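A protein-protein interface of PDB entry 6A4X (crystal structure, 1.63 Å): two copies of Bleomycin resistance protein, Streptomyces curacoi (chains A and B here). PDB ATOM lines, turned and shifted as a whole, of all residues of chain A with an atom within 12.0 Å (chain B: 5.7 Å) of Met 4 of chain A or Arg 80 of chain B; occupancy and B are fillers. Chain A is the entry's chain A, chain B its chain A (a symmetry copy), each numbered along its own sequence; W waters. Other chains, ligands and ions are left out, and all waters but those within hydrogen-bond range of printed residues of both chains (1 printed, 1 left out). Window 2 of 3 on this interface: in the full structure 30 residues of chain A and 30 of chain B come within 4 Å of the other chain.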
ATOM      1  N   MET A   4     -13.647 -24.950  16.229  1.00  0.00           N
ATOM      2  CA  MET A   4     -14.699 -25.409  15.329  1.00  0.00           C
ATOM      3  C   MET A   4     -15.668 -26.344  16.063  1.00  0.00           C
ATOM      4  O   MET A   4     -15.270 -27.398  16.562  1.00  0.00           O
ATOM      5  CB  MET A   4     -14.077 -26.093  14.104  1.00  0.00           C
ATOM      6  CG  MET A   4     -13.323 -25.119  13.193  1.00  0.00           C
ATOM      7  SD  MET A   4     -12.308 -25.867  11.897  1.00  0.00           S
ATOM      8  CE  MET A   4     -13.551 -26.537  10.798  1.00  0.00           C
ATOM      9  N   THR A   5     -16.946 -25.950  16.113  1.00  0.00           N
ATOM     10  CA  THR A   5     -17.978 -26.625  16.904  1.00  0.00           C
ATOM     11  C   THR A   5     -18.327 -28.007  16.347  1.00  0.00           C
ATOM     12  O   THR A   5     -19.447 -28.497  16.521  1.00  0.00           O
ATOM     13  CB  THR A   5     -19.226 -25.741  16.981  1.00  0.00           C
ATOM     14  OG1 THR A   5     -20.310 -26.476  17.557  1.00  0.00           O
ATOM     15  CG2 THR A   5     -19.626 -25.235  15.590  1.00  0.00           C
ATOM     16  N   VAL A   6     -17.350 -28.636  15.693  1.00  0.00           N
ATOM     17  CA  VAL A   6     -17.508 -29.945  15.067  1.00  0.00           C
ATOM     18  C   VAL A   6     -18.022 -30.975  16.064  1.00  0.00           C
ATOM     19  O   VAL A   6     -17.594 -31.008  17.221  1.00  0.00           O
ATOM     20  CB  VAL A   6     -16.144 -30.359  14.485  1.00  0.00           C
ATOM     21  CG1 VAL A   6     -16.187 -31.775  13.932  1.00  0.00           C
ATOM     22  CG2 VAL A   6     -15.691 -29.346  13.431  1.00  0.00           C
ATOM     23  N   GLN A   7     -18.929 -31.850  15.612  1.00  0.00           N
ATOM     24  CA  GLN A   7     -19.388 -32.972  16.425  1.00  0.00           C
ATOM     25  C   GLN A   7     -19.299 -34.254  15.622  1.00  0.00           C
ATOM     26  O   GLN A   7     -19.584 -34.252  14.420  1.00  0.00           O
ATOM     27  CB  GLN A   7     -20.839 -32.805  16.875  1.00  0.00           C
ATOM     28  CG  GLN A   7     -21.137 -31.516  17.601  1.00  0.00           C
ATOM     29  CD  GLN A   7     -22.613 -31.349  17.884  1.00  0.00           C
ATOM     30  OE1 GLN A   7     -23.425 -32.222  17.574  1.00  0.00           O
ATOM     31  NE2 GLN A   7     -22.973 -30.208  18.463  1.00  0.00           N
ATOM     32  N   LEU A   8     -18.913 -35.350  16.287  1.00  0.00           N
ATOM     33  CA  LEU A   8     -19.159 -36.663  15.709  1.00  0.00           C
ATOM     34  C   LEU A   8     -20.649 -36.949  15.804  1.00  0.00           C
ATOM     35  O   LEU A   8     -21.206 -37.032  16.906  1.00  0.00           O
ATOM     36  CB  LEU A   8     -18.349 -37.748  16.419  1.00  0.00           C
ATOM     37  CG  LEU A   8     -18.590 -39.152  15.869  1.00  0.00           C
ATOM     38  CD1 LEU A   8     -18.053 -39.284  14.437  1.00  0.00           C
ATOM     39  CD2 LEU A   8     -18.006 -40.250  16.773  1.00  0.00           C
ATOM     40  N   ASN A   9     -21.298 -37.092  14.652  1.00  0.00           N
ATOM     41  CA  ASN A   9     -22.749 -37.218  14.579  1.00  0.00           C
ATOM     42  C   ASN A   9     -23.234 -38.659  14.490  1.00  0.00           C
ATOM     43  O   ASN A   9     -24.264 -38.991  15.084  1.00  0.00           O
ATOM     44  CB  ASN A   9     -23.281 -36.428  13.374  1.00  0.00           C
ATOM     45  CG  ASN A   9     -24.793 -36.426  13.301  1.00  0.00           C
ATOM     46  OD1 ASN A   9     -25.460 -35.636  13.987  1.00  0.00           O
ATOM     47  ND2 ASN A   9     -25.353 -37.312  12.477  1.00  0.00           N
ATOM     48  N   ASP B  27      -6.149 -32.326  10.935  1.00  0.00           N
ATOM     49  CA  ASP B  27      -5.952 -31.200  10.025  1.00  0.00           C
ATOM     50  C   ASP B  27      -7.213 -30.908   9.214  1.00  0.00           C
ATOM     51  O   ASP B  27      -7.586 -29.742   9.041  1.00  0.00           O
ATOM     52  CB  ASP B  27      -4.768 -31.465   9.093  1.00  0.00           C
ATOM     53  CG  ASP B  27      -3.419 -31.325   9.798  1.00  0.00           C
ATOM     54  OD1 ASP B  27      -3.383 -30.831  10.947  1.00  0.00           O
ATOM     55  OD2 ASP B  27      -2.397 -31.724   9.198  1.00  0.00           O
ATOM     56  N   ILE B  28      -7.879 -31.945   8.693  1.00  0.00           N
ATOM     57  CA  ILE B  28      -9.005 -31.686   7.796  1.00  0.00           C
ATOM     58  C   ILE B  28     -10.160 -31.030   8.555  1.00  0.00           C
ATOM     59  O   ILE B  28     -10.831 -30.133   8.031  1.00  0.00           O
ATOM     60  CB  ILE B  28      -9.431 -32.977   7.061  1.00  0.00           C
ATOM     61  CG1 ILE B  28      -9.970 -32.652   5.667  1.00  0.00           C
ATOM     62  CG2 ILE B  28     -10.462 -33.789   7.850  1.00  0.00           C
ATOM     63  CD1 ILE B  28      -8.880 -32.378   4.649  1.00  0.00           C
ATOM     64  N   LEU B  29     -10.367 -31.414   9.818  1.00  0.00           N
ATOM     65  CA  LEU B  29     -11.467 -30.887  10.619  1.00  0.00           C
ATOM     66  C   LEU B  29     -11.108 -29.635  11.415  1.00  0.00           C
ATOM     67  O   LEU B  29     -11.995 -29.047  12.054  1.00  0.00           O
ATOM     68  CB  LEU B  29     -11.974 -31.964  11.587  1.00  0.00           C
ATOM     69  CG  LEU B  29     -12.589 -33.224  10.965  1.00  0.00           C
ATOM     70  CD1 LEU B  29     -13.022 -34.203  12.058  1.00  0.00           C
ATOM     71  CD2 LEU B  29     -13.767 -32.856  10.051  1.00  0.00           C
ATOM     72  N   GLY B  30      -9.844 -29.210  11.402  1.00  0.00           N
ATOM     73  CA  GLY B  30      -9.443 -28.068  12.208  1.00  0.00           C
ATOM     74  C   GLY B  30      -9.275 -28.372  13.678  1.00  0.00           C
ATOM     75  O   GLY B  30      -9.382 -27.462  14.515  1.00  0.00           O
ATOM     76  N   LEU B  31      -9.024 -29.624  14.019  1.00  0.00           N
ATOM     77  CA  LEU B  31      -8.845 -30.061  15.389  1.00  0.00           C
ATOM     78  C   LEU B  31      -7.357 -30.303  15.647  1.00  0.00           C
ATOM     79  O   LEU B  31      -6.502 -30.007  14.807  1.00  0.00           O
ATOM     80  CB  LEU B  31      -9.703 -31.307  15.640  1.00  0.00           C
ATOM     81  CG  LEU B  31     -11.210 -31.136  15.401  1.00  0.00           C
ATOM     82  CD1 LEU B  31     -11.927 -32.469  15.618  1.00  0.00           C
ATOM     83  CD2 LEU B  31     -11.812 -30.035  16.285  1.00  0.00           C
ATOM     84  N   PRO B  46     -15.103 -32.310  19.622  1.00  0.00           N
ATOM     85  CA  PRO B  46     -15.619 -31.444  20.692  1.00  0.00           C
ATOM     86  C   PRO B  46     -16.818 -31.976  21.461  1.00  0.00           C
ATOM     87  O   PRO B  46     -17.038 -31.501  22.582  1.00  0.00           O
ATOM     88  CB  PRO B  46     -15.966 -30.154  19.942  1.00  0.00           C
ATOM     89  CG  PRO B  46     -14.944 -30.097  18.878  1.00  0.00           C
ATOM     90  CD  PRO B  46     -14.733 -31.530  18.428  1.00  0.00           C
ATOM     91  N   ASP B  73     -17.726 -23.826   8.980  1.00  0.00           N
ATOM     92  CA  ASP B  73     -16.770 -24.926   9.021  1.00  0.00           C
ATOM     93  C   ASP B  73     -16.866 -25.795   7.773  1.00  0.00           C
ATOM     94  O   ASP B  73     -15.848 -26.306   7.289  1.00  0.00           O
ATOM     95  CB  ASP B  73     -17.003 -25.757  10.276  1.00  0.00           C
ATOM     96  CG  ASP B  73     -16.555 -25.045  11.540  1.00  0.00           C
ATOM     97  OD1 ASP B  73     -15.989 -23.933  11.439  1.00  0.00           O
ATOM     98  OD2 ASP B  73     -16.772 -25.600  12.633  1.00  0.00           O
ATOM     99  N   ASP B  75     -17.463 -24.802   4.727  1.00  0.00           N
ATOM    100  CA  ASP B  75     -16.671 -24.126   3.705  1.00  0.00           C
ATOM    101  C   ASP B  75     -15.178 -24.308   3.952  1.00  0.00           C
ATOM    102  O   ASP B  75     -14.414 -24.566   3.015  1.00  0.00           O
ATOM    103  CB  ASP B  75     -17.039 -22.648   3.663  1.00  0.00           C
ATOM    104  CG  ASP B  75     -18.464 -22.412   3.185  1.00  0.00           C
ATOM    105  OD1 ASP B  75     -18.910 -23.104   2.242  1.00  0.00           O
ATOM    106  OD2 ASP B  75     -19.136 -21.530   3.758  1.00  0.00           O
ATOM    107  N   THR B  76     -14.747 -24.201   5.209  1.00  0.00           N
ATOM    108  CA  THR B  76     -13.327 -24.348   5.516  1.00  0.00           C
ATOM    109  C   THR B  76     -12.847 -25.765   5.246  1.00  0.00           C
ATOM    110  O   THR B  76     -11.822 -25.965   4.583  1.00  0.00           O
ATOM    111  CB  THR B  76     -13.059 -23.969   6.967  1.00  0.00           C
ATOM    112  OG1 THR B  76     -13.469 -22.617   7.181  1.00  0.00           O
ATOM    113  CG2 THR B  76     -11.575 -24.091   7.269  1.00  0.00           C
ATOM    114  N   ILE B  77     -13.576 -26.757   5.759  1.00  0.00           N
ATOM    115  CA  ILE B  77     -13.203 -28.157   5.557  1.00  0.00           C
ATOM    116  C   ILE B  77     -13.200 -28.494   4.079  1.00  0.00           C
ATOM    117  O   ILE B  77     -12.283 -29.156   3.575  1.00  0.00           O
ATOM    118  CB  ILE B  77     -14.160 -29.079   6.334  1.00  0.00           C
ATOM    119  CG1 ILE B  77     -14.026 -28.818   7.832  1.00  0.00           C
ATOM    120  CG2 ILE B  77     -13.891 -30.540   5.997  1.00  0.00           C
ATOM    121  CD1 ILE B  77     -15.149 -29.406   8.667  1.00  0.00           C
ATOM    122  N   PHE B  78     -14.246 -28.074   3.369  1.00  0.00           N
ATOM    123  CA  PHE B  78     -14.319 -28.312   1.932  1.00  0.00           C
ATOM    124  C   PHE B  78     -13.104 -27.733   1.217  1.00  0.00           C
ATOM    125  O   PHE B  78     -12.563 -28.355   0.291  1.00  0.00           O
ATOM    126  CB  PHE B  78     -15.622 -27.721   1.396  1.00  0.00           C
ATOM    127  CG  PHE B  78     -15.969 -28.153   0.010  1.00  0.00           C
ATOM    128  CD1 PHE B  78     -16.263 -29.475  -0.266  1.00  0.00           C
ATOM    129  CD2 PHE B  78     -16.035 -27.223  -1.015  1.00  0.00           C
ATOM    130  CE1 PHE B  78     -16.594 -29.864  -1.546  1.00  0.00           C
ATOM    131  CE2 PHE B  78     -16.369 -27.605  -2.297  1.00  0.00           C
ATOM    132  CZ  PHE B  78     -16.650 -28.923  -2.563  1.00  0.00           C
ATOM    133  N   GLY B  79     -12.645 -26.551   1.645  1.00  0.00           N
ATOM    134  CA  GLY B  79     -11.424 -25.994   1.082  1.00  0.00           C
ATOM    135  C   GLY B  79     -10.218 -26.903   1.257  1.00  0.00           C
ATOM    136  O   GLY B  79      -9.431 -27.091   0.325  1.00  0.00           O
ATOM    137  N   ARG B  80     -10.059 -27.478   2.453  1.00  0.00           N
ATOM    138  CA  ARG B  80      -8.902 -28.327   2.718  1.00  0.00           C
ATOM    139  C   ARG B  80      -8.966 -29.614   1.909  1.00  0.00           C
ATOM    140  O   ARG B  80      -7.933 -30.113   1.446  1.00  0.00           O
ATOM    141  CB  ARG B  80      -8.814 -28.657   4.205  1.00  0.00           C
ATOM    142  CG  ARG B  80      -8.658 -27.463   5.120  1.00  0.00           C
ATOM    143  CD  ARG B  80      -8.485 -27.954   6.544  1.00  0.00           C
ATOM    144  NE  ARG B  80      -8.341 -26.846   7.475  1.00  0.00           N
ATOM    145  CZ  ARG B  80      -9.226 -26.518   8.411  1.00  0.00           C
ATOM    146  NH1 ARG B  80     -10.336 -27.226   8.571  1.00  0.00           N
ATOM    147  NH2 ARG B  80      -8.991 -25.471   9.193  1.00  0.00           N
ATOM    148  N   ILE B  81     -10.172 -30.165   1.734  1.00  0.00           N
ATOM    149  CA  ILE B  81     -10.339 -31.367   0.917  1.00  0.00           C
ATOM    150  C   ILE B  81      -9.864 -31.106  -0.506  1.00  0.00           C
ATOM    151  O   ILE B  81      -9.127 -31.907  -1.096  1.00  0.00           O
ATOM    152  CB  ILE B  81     -11.807 -31.832   0.950  1.00  0.00           C
ATOM    153  CG1 ILE B  81     -12.183 -32.287   2.359  1.00  0.00           C
ATOM    154  CG2 ILE B  81     -12.054 -32.960  -0.057  1.00  0.00           C
ATOM    155  CD1 ILE B  81     -13.669 -32.473   2.581  1.00  0.00           C
ATOM    156  N   ARG B  82     -10.271 -29.969  -1.075  1.00  0.00           N
ATOM    157  CA  ARG B  82      -9.854 -29.626  -2.431  1.00  0.00           C
ATOM    158  C   ARG B  82      -8.357 -29.356  -2.503  1.00  0.00           C
ATOM    159  O   ARG B  82      -7.698 -29.727  -3.487  1.00  0.00           O
ATOM    160  CB  ARG B  82     -10.649 -28.419  -2.927  1.00  0.00           C
ATOM    161  CG  ARG B  82     -12.119 -28.730  -3.181  1.00  0.00           C
ATOM    162  CD  ARG B  82     -12.845 -27.580  -3.884  1.00  0.00           C
ATOM    163  NE  ARG B  82     -13.397 -26.612  -2.939  1.00  0.00           N
ATOM    164  CZ  ARG B  82     -12.782 -25.493  -2.563  1.00  0.00           C
ATOM    165  NH1 ARG B  82     -11.586 -25.188  -3.053  1.00  0.00           N
ATOM    166  NH2 ARG B  82     -13.367 -24.674  -1.695  1.00  0.00           N
ATOM    167  N   GLU B  83      -7.802 -28.711  -1.474  1.00  0.00           N
ATOM    168  CA  GLU B  83      -6.372 -28.435  -1.452  1.00  0.00           C
ATOM    169  C   GLU B  83      -5.557 -29.719  -1.377  1.00  0.00           C
ATOM    170  O   GLU B  83      -4.404 -29.749  -1.823  1.00  0.00           O
ATOM    171  CB  GLU B  83      -6.039 -27.516  -0.276  1.00  0.00           C
ATOM    172  CG  GLU B  83      -6.274 -26.045  -0.570  1.00  0.00           C
ATOM    173  CD  GLU B  83      -6.510 -25.214   0.680  1.00  0.00           C
ATOM    174  OE1 GLU B  83      -6.197 -25.691   1.793  1.00  0.00           O
ATOM    175  OE2 GLU B  83      -7.011 -24.076   0.543  1.00  0.00           O
ATOM    176  N   ALA B  84      -6.130 -30.776  -0.818  1.00  0.00           N
ATOM    177  CA  ALA B  84      -5.462 -32.067  -0.730  1.00  0.00           C
ATOM    178  C   ALA B  84      -5.608 -32.887  -2.005  1.00  0.00           C
ATOM    179  O   ALA B  84      -5.058 -33.995  -2.081  1.00  0.00           O
ATOM    180  CB  ALA B  84      -6.006 -32.859   0.462  1.00  0.00           C
ATOM    181  N   GLY B  85      -6.337 -32.378  -2.994  1.00  0.00           N
ATOM    182  CA  GLY B  85      -6.556 -33.119  -4.219  1.00  0.00           C
ATOM    183  C   GLY B  85      -7.419 -34.347  -4.058  1.00  0.00           C
ATOM    184  O   GLY B  85      -7.315 -35.280  -4.862  1.00  0.00           O
ATOM    185  N   LEU B  86      -8.277 -34.374  -3.047  1.00  0.00           N
ATOM    186  CA  LEU B  86      -9.111 -35.533  -2.775  1.00  0.00           C
ATOM    187  C   LEU B  86     -10.398 -35.441  -3.577  1.00  0.00           C
ATOM    188  O   LEU B  86     -11.017 -34.378  -3.648  1.00  0.00           O
ATOM    189  CB  LEU B  86      -9.436 -35.639  -1.285  1.00  0.00           C
ATOM    190  CG  LEU B  86      -8.222 -35.751  -0.370  1.00  0.00           C
ATOM    191  CD1 LEU B  86      -8.673 -35.652   1.074  1.00  0.00           C
ATOM    192  CD2 LEU B  86      -7.512 -37.071  -0.636  1.00  0.00           C
HETATM  193  O   HOH W   1      -9.306 -24.807  13.552  1.00  0.00           O
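O of Leu 29 of chain B lies close to SD of Met 4 of chain A (3.2 Å).
O of Asp 27 of chain B lies close to NE of Arg 80 of chain B (3.4 Å).
O of Ile 28 of chain B sits at hydrogen-bond distance from NH1 of Arg 80 of chain B, 3.0 Å away.
Gly 30 of chain B touches Met 4 of chain A (CA to SD, 3.6 Å).
Met 4 of chain A touches Pro 46 of chain B.
CB of Met 4 of chain A touches OD2 of Asp 73 of chain B (3.1 Å).
CE of Met 4 of chain A touches CG1 of Ile 77 of chain B (3.8 Å).
NH1 of Arg 80 of chain B touches CE of Met 4 of chain A, 3.97 Å away.
OD2 of Asp 73 of chain B touches N of Thr 5 of chain A, at 3.5 Å.
Leu 29 of chain B touches Val 6 of chain A (O to CG2, 3.96 Å).
Pro 46 of chain B touches Val 6 of chain A.
Asp 73 of chain B touches Val 6 of chain A (OD2 to CG2, 3.98 Å).
Of chain B, only Leu 29, Gly 30, Pro 46, Asp 73, Ile 77 and Arg 80 come within 4 Å of Met 4 of chain A.
Of chain A, only Met 4 (3.97 Å) comes within 4 Å of Arg 80 of chain B.
No residue of chain A comes within 4 Å of Asp 27 of chain B.
No residue of chain A comes within 4 Å of Ile 28 of chain B.
No residue of chain A comes within 4 Å of Leu 31 of chain B.
Pro 46 of chain B touches just these residues of chain A: Met 4 (3.6 Å) and Val 6 (3.1 Å).
Of the printed residues of chain A, Asp 73 of chain B touches Met 4 (3.1 Å), Thr 5 (3.5 Å) and Val 6 (3.98 Å).
Ile 77 of chain B touches just one residue of chain A: Met 4.
No residue of chain A comes within 4 Å of Gly 79 of chain B.
No residue of chain A comes within 4 Å of Glu 83 of chain B.
No residue of chain A comes within 4 Å of Leu 86 of chain B.
Of the printed residues of chain B, Val 6 of chain A touches Leu 29 (3.96 Å), Pro 46 (3.1 Å) and Asp 73 (3.98 Å).
Printed residues of chain B within 4 Å of Thr 5 of chain A: Asp 73 (3.5 Å).
Asn 9 of chain A touches none of the printed residues of chain B.
The nearest printed residue of chain B that does not touch Val 6 of chain A is Leu 31 of chain B (4.6 Å).
Printed residues of chain A that touch a printed residue of chain B: Met 4, Thr 5 and Val 6.
Hydrophobic or aromatic side chains of chain A within 4 Å of the printed part of chain B: Met 4 and Val 6.
Of the 19 printed residues of chain B, 6 touch a printed residue of chain A.
Printed residues of chain B that touch a printed residue of chain A: Leu 29, Gly 30, Pro 46, Asp 73, Ile 77 and Arg 80.
Hydrophobic or aromatic side chains of chain B within 4 Å of the printed part of chain A: Pro 46 and Ile 77.
No position is printed for both chains.
Of the 10 pairs that touch across the chains among the printed residues, none has its exchanged pair printed and touching as well.
Water W1 lies within hydrogen-bond range of O of Gly 30 of chain B and SD of Met 4 of chain A.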
